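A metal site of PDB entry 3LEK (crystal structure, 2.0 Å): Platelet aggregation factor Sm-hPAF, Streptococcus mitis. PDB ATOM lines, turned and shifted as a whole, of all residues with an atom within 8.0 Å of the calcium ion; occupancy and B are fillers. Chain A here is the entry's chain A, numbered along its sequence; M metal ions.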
ATOM      1  N   ALA A  28     -12.203  12.639 -17.511  1.00  0.00           N
ATOM      2  CA  ALA A  28     -12.411  11.928 -18.792  1.00  0.00           C
ATOM      3  C   ALA A  28     -13.132  12.760 -19.839  1.00  0.00           C
ATOM      4  O   ALA A  28     -14.114  13.409 -19.511  1.00  0.00           O
ATOM      5  CB  ALA A  28     -13.215  10.621 -18.541  1.00  0.00           C
ATOM      6  N   ALA A  29     -12.618  12.724 -21.072  1.00  0.00           N
ATOM      7  CA  ALA A  29     -13.179  13.478 -22.199  1.00  0.00           C
ATOM      8  C   ALA A  29     -14.672  13.214 -22.411  1.00  0.00           C
ATOM      9  O   ALA A  29     -15.387  14.112 -22.838  1.00  0.00           O
ATOM     10  CB  ALA A  29     -12.402  13.168 -23.500  1.00  0.00           C
ATOM     11  N   THR A  30     -15.119  11.982 -22.151  1.00  0.00           N
ATOM     12  CA  THR A  30     -16.523  11.598 -22.339  1.00  0.00           C
ATOM     13  C   THR A  30     -17.472  12.364 -21.380  1.00  0.00           C
ATOM     14  O   THR A  30     -18.693  12.390 -21.604  1.00  0.00           O
ATOM     15  CB  THR A  30     -16.720  10.062 -22.159  1.00  0.00           C
ATOM     16  OG1 THR A  30     -16.143   9.643 -20.931  1.00  0.00           O
ATOM     17  CG2 THR A  30     -16.096   9.294 -23.262  1.00  0.00           C
ATOM     18  N   ARG A  31     -16.921  13.008 -20.339  1.00  0.00           N
ATOM     19  CA  ARG A  31     -17.723  13.824 -19.404  1.00  0.00           C
ATOM     20  C   ARG A  31     -18.352  15.008 -20.092  1.00  0.00           C
ATOM     21  O   ARG A  31     -19.364  15.507 -19.616  1.00  0.00           O
ATOM     22  CB  ARG A  31     -16.918  14.304 -18.177  1.00  0.00           C
ATOM     23  CG  ARG A  31     -16.701  13.216 -17.134  1.00  0.00           C
ATOM     24  CD  ARG A  31     -15.566  13.581 -16.184  1.00  0.00           C
ATOM     25  NE  ARG A  31     -15.294  12.480 -15.250  1.00  0.00           N
ATOM     26  CZ  ARG A  31     -14.761  12.644 -14.028  1.00  0.00           C
ATOM     27  NH1 ARG A  31     -14.555  11.599 -13.231  1.00  0.00           N
ATOM     28  NH2 ARG A  31     -14.423  13.861 -13.583  1.00  0.00           N
ATOM     29  N   ALA A  32     -17.779  15.455 -21.226  1.00  0.00           N
ATOM     30  CA  ALA A  32     -18.421  16.566 -21.966  1.00  0.00           C
ATOM     31  C   ALA A  32     -19.607  16.148 -22.871  1.00  0.00           C
ATOM     32  O   ALA A  32     -20.262  16.993 -23.458  1.00  0.00           O
ATOM     33  CB  ALA A  32     -17.363  17.341 -22.817  1.00  0.00           C
ATOM     34  N   VAL A  33     -19.850  14.841 -23.004  1.00  0.00           N
ATOM     35  CA  VAL A  33     -20.949  14.367 -23.842  1.00  0.00           C
ATOM     36  C   VAL A  33     -21.812  13.330 -23.111  1.00  0.00           C
ATOM     37  O   VAL A  33     -22.388  12.446 -23.744  1.00  0.00           O
ATOM     38  CB  VAL A  33     -20.474  13.836 -25.234  1.00  0.00           C
ATOM     39  CG1 VAL A  33     -19.920  15.009 -26.082  1.00  0.00           C
ATOM     40  CG2 VAL A  33     -19.443  12.694 -25.062  1.00  0.00           C
ATOM     41  N   ASP A  34     -21.896  13.463 -21.776  1.00  0.00           N
ATOM     42  CA  ASP A  34     -22.611  12.472 -20.964  1.00  0.00           C
ATOM     43  C   ASP A  34     -24.051  12.867 -20.647  1.00  0.00           C
ATOM     44  O   ASP A  34     -24.736  12.194 -19.880  1.00  0.00           O
ATOM     45  CB  ASP A  34     -21.841  12.168 -19.665  1.00  0.00           C
ATOM     46  CG  ASP A  34     -21.692  13.372 -18.726  1.00  0.00           C
ATOM     47  OD1 ASP A  34     -22.050  14.547 -19.035  1.00  0.00           O
ATOM     48  OD2 ASP A  34     -21.159  13.126 -17.617  1.00  0.00           O
ATOM     49  N   GLY A  35     -24.520  13.954 -21.255  1.00  0.00           N
ATOM     50  CA  GLY A  35     -25.896  14.428 -21.007  1.00  0.00           C
ATOM     51  C   GLY A  35     -26.098  15.062 -19.651  1.00  0.00           C
ATOM     52  O   GLY A  35     -27.223  15.110 -19.126  1.00  0.00           O
ATOM     53  N   ASN A  36     -25.018  15.583 -19.075  1.00  0.00           N
ATOM     54  CA  ASN A  36     -25.103  16.223 -17.777  1.00  0.00           C
ATOM     55  C   ASN A  36     -24.284  17.521 -17.798  1.00  0.00           C
ATOM     56  O   ASN A  36     -23.069  17.486 -17.801  1.00  0.00           O
ATOM     57  CB  ASN A  36     -24.640  15.230 -16.681  1.00  0.00           C
ATOM     58  CG  ASN A  36     -24.759  15.816 -15.260  1.00  0.00           C
ATOM     59  OD1 ASN A  36     -25.137  16.975 -15.080  1.00  0.00           O
ATOM     60  ND2 ASN A  36     -24.399  15.014 -14.257  1.00  0.00           N
ATOM     61  N   VAL A  37     -24.976  18.665 -17.806  1.00  0.00           N
ATOM     62  CA  VAL A  37     -24.303  19.961 -17.854  1.00  0.00           C
ATOM     63  C   VAL A  37     -23.823  20.499 -16.484  1.00  0.00           C
ATOM     64  O   VAL A  37     -23.338  21.628 -16.397  1.00  0.00           O
ATOM     65  CB  VAL A  37     -25.186  21.043 -18.554  1.00  0.00           C
ATOM     66  CG1 VAL A  37     -25.672  20.526 -19.913  1.00  0.00           C
ATOM     67  CG2 VAL A  37     -26.340  21.507 -17.652  1.00  0.00           C
ATOM     68  N   ASP A  38     -23.985  19.707 -15.425  1.00  0.00           N
ATOM     69  CA  ASP A  38     -23.560  20.111 -14.069  1.00  0.00           C
ATOM     70  C   ASP A  38     -22.090  20.570 -14.113  1.00  0.00           C
ATOM     71  O   ASP A  38     -21.219  19.811 -14.474  1.00  0.00           O
ATOM     72  CB  ASP A  38     -23.699  18.911 -13.122  1.00  0.00           C
ATOM     73  CG  ASP A  38     -23.528  19.293 -11.651  1.00  0.00           C
ATOM     74  OD1 ASP A  38     -24.256  18.700 -10.815  1.00  0.00           O
ATOM     75  OD2 ASP A  38     -22.676  20.144 -11.315  1.00  0.00           O
ATOM     76  N   SER A  39     -21.838  21.812 -13.727  1.00  0.00           N
ATOM     77  CA  SER A  39     -20.542  22.404 -13.984  1.00  0.00           C
ATOM     78  C   SER A  39     -19.578  22.300 -12.777  1.00  0.00           C
ATOM     79  O   SER A  39     -18.479  22.836 -12.830  1.00  0.00           O
ATOM     80  CB  SER A  39     -20.731  23.865 -14.412  1.00  0.00           C
ATOM     81  OG  SER A  39     -21.197  24.634 -13.321  1.00  0.00           O
ATOM     82  N   HIS A  43     -18.715  16.975  -9.065  1.00  0.00           N
ATOM     83  CA  HIS A  43     -19.853  16.129  -9.427  1.00  0.00           C
ATOM     84  C   HIS A  43     -19.528  15.199 -10.622  1.00  0.00           C
ATOM     85  O   HIS A  43     -20.399  14.459 -11.117  1.00  0.00           O
ATOM     86  CB  HIS A  43     -21.141  16.978  -9.649  1.00  0.00           C
ATOM     87  CG  HIS A  43     -21.558  17.772  -8.432  1.00  0.00           C
ATOM     88  ND1 HIS A  43     -22.530  18.741  -8.465  1.00  0.00           N
ATOM     89  CD2 HIS A  43     -21.108  17.733  -7.134  1.00  0.00           C
ATOM     90  CE1 HIS A  43     -22.674  19.266  -7.253  1.00  0.00           C
ATOM     91  NE2 HIS A  43     -21.835  18.674  -6.430  1.00  0.00           N
ATOM     92  N   HIS A  44     -18.257  15.245 -11.049  1.00  0.00           N
ATOM     93  CA  HIS A  44     -17.680  14.262 -11.998  1.00  0.00           C
ATOM     94  C   HIS A  44     -18.270  14.322 -13.411  1.00  0.00           C
ATOM     95  O   HIS A  44     -18.249  13.293 -14.122  1.00  0.00           O
ATOM     96  CB  HIS A  44     -17.861  12.816 -11.482  1.00  0.00           C
ATOM     97  CG  HIS A  44     -17.323  12.584 -10.112  1.00  0.00           C
ATOM     98  ND1 HIS A  44     -16.037  12.929  -9.730  1.00  0.00           N
ATOM     99  CD2 HIS A  44     -17.902  12.049  -9.006  1.00  0.00           C
ATOM    100  CE1 HIS A  44     -15.847  12.599  -8.460  1.00  0.00           C
ATOM    101  NE2 HIS A  44     -16.968  12.054  -8.001  1.00  0.00           N
ATOM    102  N   SER A  45     -18.800  15.459 -13.815  1.00  0.00           N
ATOM    103  CA  SER A  45     -19.321  15.594 -15.200  1.00  0.00           C
ATOM    104  C   SER A  45     -18.650  16.691 -16.048  1.00  0.00           C
ATOM    105  O   SER A  45     -19.222  17.145 -17.093  1.00  0.00           O
ATOM    106  CB  SER A  45     -20.842  15.768 -15.241  1.00  0.00           C
ATOM    107  OG  SER A  45     -21.274  15.401 -16.561  1.00  0.00           O
ATOM    108  N   VAL A  46     -17.420  17.017 -15.608  1.00  0.00           N
ATOM    109  CA  VAL A  46     -16.554  18.043 -16.210  1.00  0.00           C
ATOM    110  C   VAL A  46     -15.194  17.435 -16.590  1.00  0.00           C
ATOM    111  O   VAL A  46     -14.575  16.720 -15.809  1.00  0.00           O
ATOM    112  CB  VAL A  46     -16.369  19.251 -15.226  1.00  0.00           C
ATOM    113  CG1 VAL A  46     -15.533  20.413 -15.874  1.00  0.00           C
ATOM    114  CG2 VAL A  46     -17.747  19.770 -14.775  1.00  0.00           C
ATOM    115  N   THR A  47     -14.729  17.721 -17.796  1.00  0.00           N
ATOM    116  CA  THR A  47     -13.476  17.185 -18.289  1.00  0.00           C
ATOM    117  C   THR A  47     -12.305  17.978 -17.681  1.00  0.00           C
ATOM    118  O   THR A  47     -12.520  19.038 -17.057  1.00  0.00           O
ATOM    119  CB  THR A  47     -13.391  17.266 -19.851  1.00  0.00           C
ATOM    120  OG1 THR A  47     -13.195  18.640 -20.239  1.00  0.00           O
ATOM    121  CG2 THR A  47     -14.674  16.735 -20.524  1.00  0.00           C
ATOM    122  N   TYR A  73     -20.605  24.422 -22.331  1.00  0.00           N
ATOM    123  CA  TYR A  73     -20.928  24.726 -20.926  1.00  0.00           C
ATOM    124  C   TYR A  73     -19.604  24.725 -20.149  1.00  0.00           C
ATOM    125  O   TYR A  73     -18.847  23.737 -20.164  1.00  0.00           O
ATOM    126  CB  TYR A  73     -21.866  23.679 -20.358  1.00  0.00           C
ATOM    127  CG  TYR A  73     -23.234  23.644 -21.015  1.00  0.00           C
ATOM    128  CD1 TYR A  73     -24.351  24.174 -20.373  1.00  0.00           C
ATOM    129  CD2 TYR A  73     -23.406  23.049 -22.259  1.00  0.00           C
ATOM    130  CE1 TYR A  73     -25.604  24.113 -20.931  1.00  0.00           C
ATOM    131  CE2 TYR A  73     -24.648  23.020 -22.864  1.00  0.00           C
ATOM    132  CZ  TYR A  73     -25.757  23.539 -22.184  1.00  0.00           C
ATOM    133  OH  TYR A  73     -27.005  23.453 -22.766  1.00  0.00           O
ATOM    134  N   LEU A 138     -14.420  21.197 -19.715  1.00  0.00           N
ATOM    135  CA  LEU A 138     -15.752  21.504 -20.223  1.00  0.00           C
ATOM    136  C   LEU A 138     -16.785  20.677 -19.482  1.00  0.00           C
ATOM    137  O   LEU A 138     -16.642  19.475 -19.396  1.00  0.00           O
ATOM    138  CB  LEU A 138     -15.810  21.133 -21.708  1.00  0.00           C
ATOM    139  CG  LEU A 138     -14.867  21.956 -22.596  1.00  0.00           C
ATOM    140  CD1 LEU A 138     -14.408  21.165 -23.858  1.00  0.00           C
ATOM    141  CD2 LEU A 138     -15.515  23.346 -22.965  1.00  0.00           C
ATOM    142  N   ALA A 139     -17.846  21.327 -18.978  1.00  0.00           N
ATOM    143  CA  ALA A 139     -18.933  20.609 -18.301  1.00  0.00           C
ATOM    144  C   ALA A 139     -19.721  19.828 -19.348  1.00  0.00           C
ATOM    145  O   ALA A 139     -20.199  18.703 -19.104  1.00  0.00           O
ATOM    146  CB  ALA A 139     -19.820  21.613 -17.542  1.00  0.00           C
ATOM    147  N   GLU A 140     -19.838  20.401 -20.554  1.00  0.00           N
ATOM    148  CA  GLU A 140     -20.622  19.747 -21.605  1.00  0.00           C
ATOM    149  C   GLU A 140     -20.440  20.459 -22.920  1.00  0.00           C
ATOM    150  O   GLU A 140     -20.221  21.669 -22.943  1.00  0.00           O
ATOM    151  CB  GLU A 140     -22.131  19.700 -21.249  1.00  0.00           C
ATOM    152  CG  GLU A 140     -22.951  18.677 -22.137  1.00  0.00           C
ATOM    153  CD  GLU A 140     -22.869  17.238 -21.652  1.00  0.00           C
ATOM    154  OE1 GLU A 140     -22.106  16.909 -20.665  1.00  0.00           O
ATOM    155  OE2 GLU A 140     -23.580  16.397 -22.289  1.00  0.00           O
ATOM    156  N   VAL A 141     -20.424  19.673 -23.997  1.00  0.00           N
ATOM    157  CA  VAL A 141     -20.518  20.169 -25.387  1.00  0.00           C
ATOM    158  C   VAL A 141     -21.711  19.521 -26.082  1.00  0.00           C
ATOM    159  O   VAL A 141     -21.786  18.285 -26.187  1.00  0.00           O
ATOM    160  CB  VAL A 141     -19.205  19.893 -26.217  1.00  0.00           C
ATOM    161  CG1 VAL A 141     -19.330  20.464 -27.674  1.00  0.00           C
ATOM    162  CG2 VAL A 141     -17.994  20.511 -25.481  1.00  0.00           C
HETATM  163 CA    CA M   1     -21.061  16.618 -18.548  1.00  0.00          CA
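The backbone carbonyl oxygen of His 44 is in hydrogen-bond range of the guanidinium group of Arg 31, at 3.3 Å.
The backbone NH (N) of Asp 38 sits at hydrogen-bond distance from the side-chain amide oxygen (OD1) of Asn 36, 3.0 Å away.
The backbone carbonyl oxygen (O) of Tyr 73 is in hydrogen-bond range of the backbone NH (N) of Ala 139, 2.9 Å away.
The backbone NH of Gly 35 sits at hydrogen-bond distance from the side-chain carboxylate of Glu 140, 2.8 Å away.
O of Glu 140 lies within hydrogen-bond range of N of Tyr 73.
Within 4 Å of the calcium ion: Arg 31, Asp 34, Asn 36, Ser 45, Ala 139 and Glu 140.
The nearest printed residue that does not touch the calcium ion is Ala 32 (4.3 Å).
The calcium ion is bound by O of Arg 31 (2.3 Å), O of Asn 36 (2.3 Å), O of Ala 139 (2.3 Å), OG of Ser 45 (2.3 Å), OD1 of Asp 34 (2.3 Å), OE1 of Glu 140 (2.4 Å) and O of Ser 45 (2.4 Å).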
